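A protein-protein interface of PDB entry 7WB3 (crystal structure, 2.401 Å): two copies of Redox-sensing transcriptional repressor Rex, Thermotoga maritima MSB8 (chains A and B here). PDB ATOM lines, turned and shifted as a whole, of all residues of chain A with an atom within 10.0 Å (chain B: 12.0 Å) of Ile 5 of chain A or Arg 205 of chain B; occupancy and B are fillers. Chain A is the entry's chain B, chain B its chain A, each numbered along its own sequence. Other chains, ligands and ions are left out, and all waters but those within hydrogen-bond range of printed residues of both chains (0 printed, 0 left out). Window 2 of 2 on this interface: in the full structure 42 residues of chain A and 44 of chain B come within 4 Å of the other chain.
The side-chain hydroxyl (OG1) of Thr 200 of chain B is in hydrogen-bond range of the backbone carbonyl oxygen (O) of Leu 77 of chain A (2.7 Å). O of Leu 77 of chain A is in hydrogen-bond range of N of Phe 201 of chain B (3.5 Å).
The backbone carbonyl oxygen (O) of Arg 197 of chain B sits at hydrogen-bond distance from the side-chain hydroxyl (OG1) of Thr 200 of chain B, 2.9 Å away. The backbone carbonyl oxygen of Gly 78 of chain A sits at hydrogen-bond distance from the indole nitrogen of Trp 83 of chain A, at 2.7 Å.
Among the printed residues, pairs that only touch across the chains: Pro 186 of chain A with Arg 206 of chain B, Ile 5 of chain A with Arg 205 of chain B, Pro 186 of chain A with Glu 202 of chain B, Lys 171 of chain A with Ile 203 of chain B, Trp 83 of chain A with Ile 203 of chain B, Trp 83 of chain A with Thr 200 of chain B, Ser 10 of chain A with Phe 201 of chain B, Ile 76 of chain A with Val 204 of chain B, Ser 10 of chain A with Val 198 of chain B, Pro 186 of chain A with Leu 199 of chain B, Ile 76 of chain A with Phe 201 of chain B, Ile 5 of chain A with Phe 201 of chain B and Gly 78 of chain A with Val 204 of chain B.
Ile 5 of chain A touches two residues of chain B. No residue of chain B comes within 4 Å of Pro 6 of chain A. No residue of chain B comes within 4 Å of Val 9 of chain A. No residue of chain B comes within 4 Å of Tyr 53 of chain A. Of the printed residues of chain A, Glu 202 of chain B touches Pro 186. Printed residues of chain B within 4 Å of Ser 10 of chain A: Val 198 and Phe 201. Of the printed residues of chain B, Leu 77 of chain A touches Thr 200 (2.7 Å) and Phe 201 (3.5 Å). Of the printed residues of chain B, Pro 186 of chain A touches Leu 199 (3.8 Å), Glu 202 (3.4 Å) and Arg 206 (3.3 Å). Phe 54 of chain A touches none of the printed residues of chain B. Leu 51 of chain A touches none of the printed residues of chain B.
Printed residues of chain A that touch a printed residue of chain B: Ile 5, Ser 10, Ile 76, Leu 77, Gly 78, Trp 83, Lys 171 and Pro 186. Hydrophobic or aromatic side chains of chain A that line the printed part of chain B: Ile 5, Ile 76, Trp 83 and Pro 186. Of the 12 printed residues of chain B, 9 touch a printed residue of chain A. Hydrophobic or aromatic side chains of chain B that line the printed part of chain A: Val 198, Leu 199, Phe 201, Ile 203 and Val 204. Among the printed residues, 15 pairs touch across the chains.
No position is printed for both chains.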
ATOM      1  N   ILE A   5       6.641 -16.122 -13.502  1.00  0.00           N
ATOM      2  CA  ILE A   5       6.396 -16.813 -14.762  1.00  0.00           C
ATOM      3  C   ILE A   5       5.964 -18.250 -14.492  1.00  0.00           C
ATOM      4  O   ILE A   5       6.618 -18.968 -13.734  1.00  0.00           O
ATOM      5  CB  ILE A   5       7.640 -16.763 -15.673  1.00  0.00           C
ATOM      6  CG1 ILE A   5       8.829 -17.467 -15.013  1.00  0.00           C
ATOM      7  CG2 ILE A   5       8.000 -15.322 -16.004  1.00  0.00           C
ATOM      8  CD1 ILE A   5       8.940 -18.941 -15.347  1.00  0.00           C
ATOM      9  N   PRO A   6       4.854 -18.665 -15.100  1.00  0.00           N
ATOM     10  CA  PRO A   6       4.361 -20.030 -14.885  1.00  0.00           C
ATOM     11  C   PRO A   6       5.402 -21.070 -15.274  1.00  0.00           C
ATOM     12  O   PRO A   6       6.252 -20.844 -16.139  1.00  0.00           O
ATOM     13  CB  PRO A   6       3.125 -20.107 -15.786  1.00  0.00           C
ATOM     14  CG  PRO A   6       2.672 -18.690 -15.911  1.00  0.00           C
ATOM     15  CD  PRO A   6       3.930 -17.869 -15.927  1.00  0.00           C
ATOM     16  N   LYS A   7       5.323 -22.227 -14.619  1.00  0.00           N
ATOM     17  CA  LYS A   7       6.332 -23.262 -14.821  1.00  0.00           C
ATOM     18  C   LYS A   7       6.342 -23.832 -16.234  1.00  0.00           C
ATOM     19  O   LYS A   7       7.441 -24.040 -16.777  1.00  0.00           O
ATOM     20  CB  LYS A   7       6.129 -24.383 -13.793  1.00  0.00           C
ATOM     21  CG  LYS A   7       6.089 -23.907 -12.349  1.00  0.00           C
ATOM     22  CD  LYS A   7       5.645 -25.024 -11.414  1.00  0.00           C
ATOM     23  CE  LYS A   7       5.699 -24.585  -9.961  1.00  0.00           C
ATOM     24  NZ  LYS A   7       5.314 -25.687  -9.038  1.00  0.00           N
ATOM     25  N   PRO A   8       5.203 -24.114 -16.875  1.00  0.00           N
ATOM     26  CA  PRO A   8       5.244 -24.719 -18.217  1.00  0.00           C
ATOM     27  C   PRO A   8       5.704 -23.773 -19.315  1.00  0.00           C
ATOM     28  O   PRO A   8       5.868 -24.222 -20.457  1.00  0.00           O
ATOM     29  CB  PRO A   8       3.794 -25.164 -18.444  1.00  0.00           C
ATOM     30  CG  PRO A   8       2.986 -24.259 -17.580  1.00  0.00           C
ATOM     31  CD  PRO A   8       3.825 -24.004 -16.361  1.00  0.00           C
ATOM     32  N   VAL A   9       5.918 -22.490 -19.016  1.00  0.00           N
ATOM     33  CA  VAL A   9       6.246 -21.528 -20.065  1.00  0.00           C
ATOM     34  C   VAL A   9       7.631 -21.807 -20.639  1.00  0.00           C
ATOM     35  O   VAL A   9       7.817 -21.853 -21.860  1.00  0.00           O
ATOM     36  CB  VAL A   9       6.137 -20.089 -19.528  1.00  0.00           C
ATOM     37  CG1 VAL A   9       6.582 -19.094 -20.587  1.00  0.00           C
ATOM     38  CG2 VAL A   9       4.713 -19.795 -19.080  1.00  0.00           C
ATOM     39  N   SER A  10       8.627 -21.986 -19.765  1.00  0.00           N
ATOM     40  CA  SER A  10       9.999 -22.176 -20.229  1.00  0.00           C
ATOM     41  C   SER A  10      10.090 -23.300 -21.255  1.00  0.00           C
ATOM     42  O   SER A  10      10.802 -23.181 -22.259  1.00  0.00           O
ATOM     43  CB  SER A  10      10.920 -22.462 -19.042  1.00  0.00           C
ATOM     44  OG  SER A  10      10.615 -23.713 -18.450  1.00  0.00           O
ATOM     45  N   LYS A  11       9.373 -24.400 -21.018  1.00  0.00           N
ATOM     46  CA  LYS A  11       9.397 -25.513 -21.960  1.00  0.00           C
ATOM     47  C   LYS A  11       8.869 -25.082 -23.323  1.00  0.00           C
ATOM     48  O   LYS A  11       9.475 -25.374 -24.359  1.00  0.00           O
ATOM     49  CB  LYS A  11       8.582 -26.683 -21.406  1.00  0.00           C
ATOM     50  CG  LYS A  11       8.984 -28.042 -21.949  1.00  0.00           C
ATOM     51  CD  LYS A  11       8.211 -29.155 -21.256  1.00  0.00           C
ATOM     52  CE  LYS A  11       8.501 -30.510 -21.882  1.00  0.00           C
ATOM     53  NZ  LYS A  11       9.932 -30.893 -21.740  1.00  0.00           N
ATOM     54  N   ARG A  12       7.734 -24.378 -23.338  1.00  0.00           N
ATOM     55  CA  ARG A  12       7.177 -23.917 -24.604  1.00  0.00           C
ATOM     56  C   ARG A  12       8.062 -22.863 -25.259  1.00  0.00           C
ATOM     57  O   ARG A  12       8.122 -22.790 -26.492  1.00  0.00           O
ATOM     58  CB  ARG A  12       5.762 -23.379 -24.392  1.00  0.00           C
ATOM     59  CG  ARG A  12       4.749 -24.456 -24.033  1.00  0.00           C
ATOM     60  CD  ARG A  12       3.318 -23.956 -24.164  1.00  0.00           C
ATOM     61  NE  ARG A  12       3.007 -22.894 -23.211  1.00  0.00           N
ATOM     62  CZ  ARG A  12       2.452 -23.099 -22.020  1.00  0.00           C
ATOM     63  NH1 ARG A  12       2.148 -24.330 -21.631  1.00  0.00           N
ATOM     64  NH2 ARG A  12       2.200 -22.074 -21.219  1.00  0.00           N
ATOM     65  N   LEU A  13       8.756 -22.046 -24.462  1.00  0.00           N
ATOM     66  CA  LEU A  13       9.681 -21.074 -25.036  1.00  0.00           C
ATOM     67  C   LEU A  13      10.754 -21.764 -25.868  1.00  0.00           C
ATOM     68  O   LEU A  13      11.086 -21.309 -26.970  1.00  0.00           O
ATOM     69  CB  LEU A  13      10.330 -20.239 -23.932  1.00  0.00           C
ATOM     70  CG  LEU A  13       9.640 -18.959 -23.464  1.00  0.00           C
ATOM     71  CD1 LEU A  13      10.488 -18.270 -22.407  1.00  0.00           C
ATOM     72  CD2 LEU A  13       9.381 -18.027 -24.636  1.00  0.00           C
ATOM     73  N   LYS A  49       0.244 -15.219 -24.951  1.00  0.00           N
ATOM     74  CA  LYS A  49       0.321 -15.036 -23.505  1.00  0.00           C
ATOM     75  C   LYS A  49       1.733 -15.296 -22.994  1.00  0.00           C
ATOM     76  O   LYS A  49       2.295 -14.488 -22.245  1.00  0.00           O
ATOM     77  CB  LYS A  49      -0.682 -15.957 -22.809  1.00  0.00           C
ATOM     78  CG  LYS A  49      -0.677 -15.851 -21.293  1.00  0.00           C
ATOM     79  CD  LYS A  49      -1.090 -14.464 -20.829  1.00  0.00           C
ATOM     80  CE  LYS A  49      -2.597 -14.284 -20.927  1.00  0.00           C
ATOM     81  NZ  LYS A  49      -3.049 -12.981 -20.368  1.00  0.00           N
ATOM     82  N   ASP A  50       2.327 -16.424 -23.396  1.00  0.00           N
ATOM     83  CA  ASP A  50       3.669 -16.757 -22.927  1.00  0.00           C
ATOM     84  C   ASP A  50       4.666 -15.660 -23.276  1.00  0.00           C
ATOM     85  O   ASP A  50       5.499 -15.280 -22.445  1.00  0.00           O
ATOM     86  CB  ASP A  50       4.111 -18.097 -23.513  1.00  0.00           C
ATOM     87  CG  ASP A  50       3.262 -19.255 -23.024  1.00  0.00           C
ATOM     88  OD1 ASP A  50       2.643 -19.127 -21.945  1.00  0.00           O
ATOM     89  OD2 ASP A  50       3.217 -20.297 -23.713  1.00  0.00           O
ATOM     90  N   LEU A  51       4.601 -15.139 -24.504  1.00  0.00           N
ATOM     91  CA  LEU A  51       5.487 -14.043 -24.882  1.00  0.00           C
ATOM     92  C   LEU A  51       5.184 -12.781 -24.085  1.00  0.00           C
ATOM     93  O   LEU A  51       6.079 -11.956 -23.866  1.00  0.00           O
ATOM     94  CB  LEU A  51       5.370 -13.765 -26.380  1.00  0.00           C
ATOM     95  CG  LEU A  51       5.719 -14.919 -27.323  1.00  0.00           C
ATOM     96  CD1 LEU A  51       5.529 -14.495 -28.772  1.00  0.00           C
ATOM     97  CD2 LEU A  51       7.144 -15.396 -27.086  1.00  0.00           C
ATOM     98  N   SER A  52       3.934 -12.620 -23.642  1.00  0.00           N
ATOM     99  CA  SER A  52       3.559 -11.442 -22.866  1.00  0.00           C
ATOM    100  C   SER A  52       4.374 -11.320 -21.586  1.00  0.00           C
ATOM    101  O   SER A  52       4.655 -10.205 -21.134  1.00  0.00           O
ATOM    102  CB  SER A  52       2.066 -11.489 -22.539  1.00  0.00           C
ATOM    103  OG  SER A  52       1.705 -10.444 -21.654  1.00  0.00           O
ATOM    104  N   TYR A  53       4.755 -12.449 -20.982  1.00  0.00           N
ATOM    105  CA  TYR A  53       5.483 -12.405 -19.719  1.00  0.00           C
ATOM    106  C   TYR A  53       6.824 -11.695 -19.843  1.00  0.00           C
ATOM    107  O   TYR A  53       7.334 -11.182 -18.841  1.00  0.00           O
ATOM    108  CB  TYR A  53       5.706 -13.822 -19.182  1.00  0.00           C
ATOM    109  CG  TYR A  53       4.438 -14.553 -18.814  1.00  0.00           C
ATOM    110  CD1 TYR A  53       3.668 -14.147 -17.732  1.00  0.00           C
ATOM    111  CD2 TYR A  53       4.016 -15.658 -19.538  1.00  0.00           C
ATOM    112  CE1 TYR A  53       2.508 -14.815 -17.388  1.00  0.00           C
ATOM    113  CE2 TYR A  53       2.859 -16.334 -19.203  1.00  0.00           C
ATOM    114  CZ  TYR A  53       2.110 -15.908 -18.128  1.00  0.00           C
ATOM    115  OH  TYR A  53       0.958 -16.579 -17.793  1.00  0.00           O
ATOM    116  N   PHE A  54       7.408 -11.658 -21.042  1.00  0.00           N
ATOM    117  CA  PHE A  54       8.759 -11.148 -21.216  1.00  0.00           C
ATOM    118  C   PHE A  54       8.836  -9.842 -21.992  1.00  0.00           C
ATOM    119  O   PHE A  54       9.853  -9.149 -21.894  1.00  0.00           O
ATOM    120  CB  PHE A  54       9.631 -12.199 -21.918  1.00  0.00           C
ATOM    121  CG  PHE A  54       9.590 -13.549 -21.263  1.00  0.00           C
ATOM    122  CD1 PHE A  54      10.472 -13.865 -20.243  1.00  0.00           C
ATOM    123  CD2 PHE A  54       8.665 -14.497 -21.660  1.00  0.00           C
ATOM    124  CE1 PHE A  54      10.435 -15.108 -19.636  1.00  0.00           C
ATOM    125  CE2 PHE A  54       8.624 -15.742 -21.060  1.00  0.00           C
ATOM    126  CZ  PHE A  54       9.509 -16.046 -20.045  1.00  0.00           C
ATOM    127  N   GLY A  55       7.808  -9.489 -22.749  1.00  0.00           N
ATOM    128  CA  GLY A  55       7.802  -8.221 -23.445  1.00  0.00           C
ATOM    129  C   GLY A  55       6.780  -8.216 -24.566  1.00  0.00           C
ATOM    130  O   GLY A  55       5.998  -9.152 -24.728  1.00  0.00           O
ATOM    131  N   GLU A  75      17.924 -14.594 -26.077  1.00  0.00           N
ATOM    132  CA  GLU A  75      18.447 -13.822 -24.956  1.00  0.00           C
ATOM    133  C   GLU A  75      17.789 -14.244 -23.649  1.00  0.00           C
ATOM    134  O   GLU A  75      18.459 -14.348 -22.615  1.00  0.00           O
ATOM    135  CB  GLU A  75      18.234 -12.330 -25.213  1.00  0.00           C
ATOM    136  CG  GLU A  75      19.138 -11.406 -24.417  1.00  0.00           C
ATOM    137  CD  GLU A  75      19.128  -9.987 -24.958  1.00  0.00           C
ATOM    138  OE1 GLU A  75      19.662  -9.767 -26.066  1.00  0.00           O
ATOM    139  OE2 GLU A  75      18.582  -9.091 -24.277  1.00  0.00           O
ATOM    140  N   ILE A  76      16.480 -14.498 -23.676  1.00  0.00           N
ATOM    141  CA  ILE A  76      15.779 -14.938 -22.474  1.00  0.00           C
ATOM    142  C   ILE A  76      16.260 -16.320 -22.051  1.00  0.00           C
ATOM    143  O   ILE A  76      16.475 -16.580 -20.862  1.00  0.00           O
ATOM    144  CB  ILE A  76      14.258 -14.917 -22.703  1.00  0.00           C
ATOM    145  CG1 ILE A  76      13.761 -13.480 -22.870  1.00  0.00           C
ATOM    146  CG2 ILE A  76      13.537 -15.606 -21.555  1.00  0.00           C
ATOM    147  CD1 ILE A  76      12.316 -13.387 -23.314  1.00  0.00           C
ATOM    148  N   LEU A  77      16.429 -17.226 -23.012  1.00  0.00           N
ATOM    149  CA  LEU A  77      16.885 -18.581 -22.724  1.00  0.00           C
ATOM    150  C   LEU A  77      18.358 -18.645 -22.347  1.00  0.00           C
ATOM    151  O   LEU A  77      18.838 -19.730 -21.998  1.00  0.00           O
ATOM    152  CB  LEU A  77      16.623 -19.484 -23.931  1.00  0.00           C
ATOM    153  CG  LEU A  77      15.158 -19.695 -24.316  1.00  0.00           C
ATOM    154  CD1 LEU A  77      15.045 -20.552 -25.570  1.00  0.00           C
ATOM    155  CD2 LEU A  77      14.384 -20.316 -23.163  1.00  0.00           C
ATOM    156  N   GLY A  78      19.080 -17.529 -22.400  1.00  0.00           N
ATOM    157  CA  GLY A  78      20.504 -17.559 -22.139  1.00  0.00           C
ATOM    158  C   GLY A  78      21.316 -18.276 -23.190  1.00  0.00           C
ATOM    159  O   GLY A  78      22.431 -18.720 -22.901  1.00  0.00           O
ATOM    160  N   VAL A  79      20.790 -18.397 -24.413  1.00  0.00           N
ATOM    161  CA  VAL A  79      21.475 -19.129 -25.476  1.00  0.00           C
ATOM    162  C   VAL A  79      22.427 -18.251 -26.275  1.00  0.00           C
ATOM    163  O   VAL A  79      23.166 -18.767 -27.129  1.00  0.00           O
ATOM    164  CB  VAL A  79      20.453 -19.784 -26.428  1.00  0.00           C
ATOM    165  CG1 VAL A  79      21.155 -20.658 -27.457  1.00  0.00           C
ATOM    166  CG2 VAL A  79      19.433 -20.594 -25.638  1.00  0.00           C
ATOM    167  N   TRP A  83      28.198 -22.259 -23.663  1.00  0.00           N
ATOM    168  CA  TRP A  83      28.158 -22.863 -22.339  1.00  0.00           C
ATOM    169  C   TRP A  83      29.165 -24.001 -22.268  1.00  0.00           C
ATOM    170  O   TRP A  83      29.183 -24.876 -23.140  1.00  0.00           O
ATOM    171  CB  TRP A  83      26.752 -23.369 -22.015  1.00  0.00           C
ATOM    172  CG  TRP A  83      25.754 -22.267 -21.847  1.00  0.00           C
ATOM    173  CD1 TRP A  83      25.073 -21.621 -22.837  1.00  0.00           C
ATOM    174  CD2 TRP A  83      25.321 -21.681 -20.614  1.00  0.00           C
ATOM    175  NE1 TRP A  83      24.244 -20.668 -22.296  1.00  0.00           N
ATOM    176  CE2 TRP A  83      24.378 -20.684 -20.933  1.00  0.00           C
ATOM    177  CE3 TRP A  83      25.640 -21.901 -19.271  1.00  0.00           C
ATOM    178  CZ2 TRP A  83      23.750 -19.910 -19.959  1.00  0.00           C
ATOM    179  CZ3 TRP A  83      25.016 -21.130 -18.305  1.00  0.00           C
ATOM    180  CH2 TRP A  83      24.082 -20.148 -18.655  1.00  0.00           C
ATOM    181  N   LYS A 171      27.032 -24.139 -12.180  1.00  0.00           N
ATOM    182  CA  LYS A 171      25.840 -23.300 -12.198  1.00  0.00           C
ATOM    183  C   LYS A 171      24.555 -24.088 -12.410  1.00  0.00           C
ATOM    184  O   LYS A 171      23.475 -23.589 -12.072  1.00  0.00           O
ATOM    185  CB  LYS A 171      25.955 -22.233 -13.293  1.00  0.00           C
ATOM    186  CG  LYS A 171      27.052 -21.206 -13.060  1.00  0.00           C
ATOM    187  CD  LYS A 171      27.084 -20.189 -14.192  1.00  0.00           C
ATOM    188  CE  LYS A 171      28.248 -19.223 -14.046  1.00  0.00           C
ATOM    189  NZ  LYS A 171      28.340 -18.292 -15.207  1.00  0.00           N
ATOM    190  N   PRO A 186      20.083 -24.999 -10.107  1.00  0.00           N
ATOM    191  CA  PRO A 186      18.996 -25.617 -10.872  1.00  0.00           C
ATOM    192  C   PRO A 186      19.385 -27.003 -11.362  1.00  0.00           C
ATOM    193  O   PRO A 186      20.555 -27.292 -11.621  1.00  0.00           O
ATOM    194  CB  PRO A 186      18.786 -24.649 -12.041  1.00  0.00           C
ATOM    195  CG  PRO A 186      19.360 -23.348 -11.567  1.00  0.00           C
ATOM    196  CD  PRO A 186      20.515 -23.719 -10.690  1.00  0.00           C
ATOM    197  N   LEU B 196      18.512 -28.912 -21.835  1.00  0.00           N
ATOM    198  CA  LEU B 196      19.630 -28.001 -21.610  1.00  0.00           C
ATOM    199  C   LEU B 196      19.184 -26.547 -21.699  1.00  0.00           C
ATOM    200  O   LEU B 196      19.587 -25.716 -20.876  1.00  0.00           O
ATOM    201  CB  LEU B 196      20.747 -28.279 -22.615  1.00  0.00           C
ATOM    202  CG  LEU B 196      21.583 -29.542 -22.400  1.00  0.00           C
ATOM    203  CD1 LEU B 196      22.465 -29.812 -23.607  1.00  0.00           C
ATOM    204  CD2 LEU B 196      22.429 -29.411 -21.144  1.00  0.00           C
ATOM    205  N   ARG B 197      18.350 -26.221 -22.689  1.00  0.00           N
ATOM    206  CA  ARG B 197      17.916 -24.838 -22.855  1.00  0.00           C
ATOM    207  C   ARG B 197      16.919 -24.426 -21.778  1.00  0.00           C
ATOM    208  O   ARG B 197      16.842 -23.244 -21.429  1.00  0.00           O
ATOM    209  CB  ARG B 197      17.329 -24.642 -24.253  1.00  0.00           C
ATOM    210  CG  ARG B 197      18.395 -24.590 -25.337  1.00  0.00           C
ATOM    211  CD  ARG B 197      17.812 -24.666 -26.735  1.00  0.00           C
ATOM    212  NE  ARG B 197      18.845 -24.479 -27.749  1.00  0.00           N
ATOM    213  CZ  ARG B 197      18.690 -24.765 -29.038  1.00  0.00           C
ATOM    214  NH1 ARG B 197      17.540 -25.260 -29.475  1.00  0.00           N
ATOM    215  NH2 ARG B 197      19.687 -24.561 -29.887  1.00  0.00           N
ATOM    216  N   VAL B 198      16.151 -25.376 -21.242  1.00  0.00           N
ATOM    217  CA  VAL B 198      15.375 -25.082 -20.044  1.00  0.00           C
ATOM    218  C   VAL B 198      16.306 -24.859 -18.862  1.00  0.00           C
ATOM    219  O   VAL B 198      16.018 -24.043 -17.979  1.00  0.00           O
ATOM    220  CB  VAL B 198      14.365 -26.208 -19.760  1.00  0.00           C
ATOM    221  CG1 VAL B 198      13.660 -25.961 -18.435  1.00  0.00           C
ATOM    222  CG2 VAL B 198      13.359 -26.314 -20.893  1.00  0.00           C
ATOM    223  N   LEU B 199      17.434 -25.572 -18.827  1.00  0.00           N
ATOM    224  CA  LEU B 199      18.395 -25.400 -17.744  1.00  0.00           C
ATOM    225  C   LEU B 199      19.059 -24.030 -17.816  1.00  0.00           C
ATOM    226  O   LEU B 199      19.183 -23.336 -16.801  1.00  0.00           O
ATOM    227  CB  LEU B 199      19.445 -26.513 -17.793  1.00  0.00           C
ATOM    228  CG  LEU B 199      20.525 -26.501 -16.710  1.00  0.00           C
ATOM    229  CD1 LEU B 199      19.903 -26.489 -15.319  1.00  0.00           C
ATOM    230  CD2 LEU B 199      21.453 -27.694 -16.873  1.00  0.00           C
ATOM    231  N   THR B 200      19.495 -23.625 -19.012  1.00  0.00           N
ATOM    232  CA  THR B 200      20.100 -22.305 -19.157  1.00  0.00           C
ATOM    233  C   THR B 200      19.104 -21.210 -18.804  1.00  0.00           C
ATOM    234  O   THR B 200      19.476 -20.187 -18.217  1.00  0.00           O
ATOM    235  CB  THR B 200      20.629 -22.114 -20.578  1.00  0.00           C
ATOM    236  OG1 THR B 200      19.557 -22.270 -21.516  1.00  0.00           O
ATOM    237  CG2 THR B 200      21.721 -23.128 -20.884  1.00  0.00           C
ATOM    238  N   PHE B 201      17.832 -21.406 -19.155  1.00  0.00           N
ATOM    239  CA  PHE B 201      16.798 -20.460 -18.750  1.00  0.00           C
ATOM    240  C   PHE B 201      16.803 -20.265 -17.241  1.00  0.00           C
ATOM    241  O   PHE B 201      16.836 -19.134 -16.746  1.00  0.00           O
ATOM    242  CB  PHE B 201      15.428 -20.944 -19.229  1.00  0.00           C
ATOM    243  CG  PHE B 201      14.276 -20.158 -18.671  1.00  0.00           C
ATOM    244  CD1 PHE B 201      13.852 -18.994 -19.289  1.00  0.00           C
ATOM    245  CD2 PHE B 201      13.614 -20.585 -17.532  1.00  0.00           C
ATOM    246  CE1 PHE B 201      12.791 -18.267 -18.780  1.00  0.00           C
ATOM    247  CE2 PHE B 201      12.551 -19.861 -17.017  1.00  0.00           C
ATOM    248  CZ  PHE B 201      12.139 -18.702 -17.642  1.00  0.00           C
ATOM    249  N   GLU B 202      16.776 -21.369 -16.491  1.00  0.00           N
ATOM    250  CA  GLU B 202      16.767 -21.278 -15.036  1.00  0.00           C
ATOM    251  C   GLU B 202      18.067 -20.699 -14.498  1.00  0.00           C
ATOM    252  O   GLU B 202      18.056 -19.995 -13.481  1.00  0.00           O
ATOM    253  CB  GLU B 202      16.506 -22.655 -14.425  1.00  0.00           C
ATOM    254  CG  GLU B 202      15.129 -23.221 -14.730  1.00  0.00           C
ATOM    255  CD  GLU B 202      14.997 -24.680 -14.331  1.00  0.00           C
ATOM    256  OE1 GLU B 202      16.024 -25.298 -13.980  1.00  0.00           O
ATOM    257  OE2 GLU B 202      13.865 -25.208 -14.366  1.00  0.00           O
ATOM    258  N   ILE B 203      19.193 -20.979 -15.158  1.00  0.00           N
ATOM    259  CA  ILE B 203      20.481 -20.487 -14.674  1.00  0.00           C
ATOM    260  C   ILE B 203      20.525 -18.965 -14.731  1.00  0.00           C
ATOM    261  O   ILE B 203      20.845 -18.296 -13.740  1.00  0.00           O
ATOM    262  CB  ILE B 203      21.633 -21.115 -15.477  1.00  0.00           C
ATOM    263  CG1 ILE B 203      21.830 -22.578 -15.073  1.00  0.00           C
ATOM    264  CG2 ILE B 203      22.916 -20.320 -15.283  1.00  0.00           C
ATOM    265  CD1 ILE B 203      22.758 -23.347 -15.984  1.00  0.00           C
ATOM    266  N   VAL B 204      20.207 -18.393 -15.894  1.00  0.00           N
ATOM    267  CA  VAL B 204      20.256 -16.943 -16.042  1.00  0.00           C
ATOM    268  C   VAL B 204      19.135 -16.255 -15.273  1.00  0.00           C
ATOM    269  O   VAL B 204      19.272 -15.083 -14.906  1.00  0.00           O
ATOM    270  CB  VAL B 204      20.212 -16.553 -17.531  1.00  0.00           C
ATOM    271  CG1 VAL B 204      21.402 -17.146 -18.269  1.00  0.00           C
ATOM    272  CG2 VAL B 204      18.904 -17.008 -18.162  1.00  0.00           C
ATOM    273  N   ARG B 205      18.026 -16.952 -15.016  1.00  0.00           N
ATOM    274  CA  ARG B 205      16.949 -16.358 -14.230  1.00  0.00           C
ATOM    275  C   ARG B 205      17.386 -16.129 -12.788  1.00  0.00           C
ATOM    276  O   ARG B 205      17.262 -15.017 -12.261  1.00  0.00           O
ATOM    277  CB  ARG B 205      15.705 -17.246 -14.286  1.00  0.00           C
ATOM    278  CG  ARG B 205      14.866 -17.053 -15.542  1.00  0.00           C
ATOM    279  CD  ARG B 205      14.052 -15.765 -15.507  1.00  0.00           C
ATOM    280  NE  ARG B 205      12.865 -15.870 -14.662  1.00  0.00           N
ATOM    281  CZ  ARG B 205      11.913 -14.944 -14.598  1.00  0.00           C
ATOM    282  NH1 ARG B 205      12.008 -13.841 -15.329  1.00  0.00           N
ATOM    283  NH2 ARG B 205      10.865 -15.119 -13.805  1.00  0.00           N
ATOM    284  N   ARG B 206      17.898 -17.173 -12.131  1.00  0.00           N
ATOM    285  CA  ARG B 206      18.373 -17.028 -10.757  1.00  0.00           C
ATOM    286  C   ARG B 206      19.376 -15.888 -10.642  1.00  0.00           C
ATOM    287  O   ARG B 206      19.221 -14.984  -9.814  1.00  0.00           O
ATOM    288  CB  ARG B 206      18.998 -18.336 -10.268  1.00  0.00           C
ATOM    289  CG  ARG B 206      18.021 -19.485 -10.080  1.00  0.00           C
ATOM    290  CD  ARG B 206      18.646 -20.582  -9.228  1.00  0.00           C
ATOM    291  NE  ARG B 206      17.800 -21.769  -9.130  1.00  0.00           N
ATOM    292  CZ  ARG B 206      18.051 -22.799  -8.327  1.00  0.00           C
ATOM    293  NH1 ARG B 206      19.122 -22.785  -7.546  1.00  0.00           N
ATOM    294  NH2 ARG B 206      17.232 -23.842  -8.302  1.00  0.00           N
ATOM    295  N   ASN B 207      20.417 -15.918 -11.469  1.00  0.00           N
ATOM    296  CA  ASN B 207      21.436 -14.875 -11.461  1.00  0.00           C
ATOM    297  C   ASN B 207      20.996 -13.678 -12.298  1.00  0.00           C
ATOM    298  O   ASN B 207      20.747 -12.596 -11.769  1.00  0.00           O
ATOM    299  CB  ASN B 207      22.767 -15.421 -11.980  1.00  0.00           C
ATOM    300  CG  ASN B 207      23.859 -14.370 -12.002  1.00  0.00           C
ATOM    301  OD1 ASN B 207      23.824 -13.407 -11.237  1.00  0.00           O
ATOM    302  ND2 ASN B 207      24.834 -14.549 -12.887  1.00  0.00           N
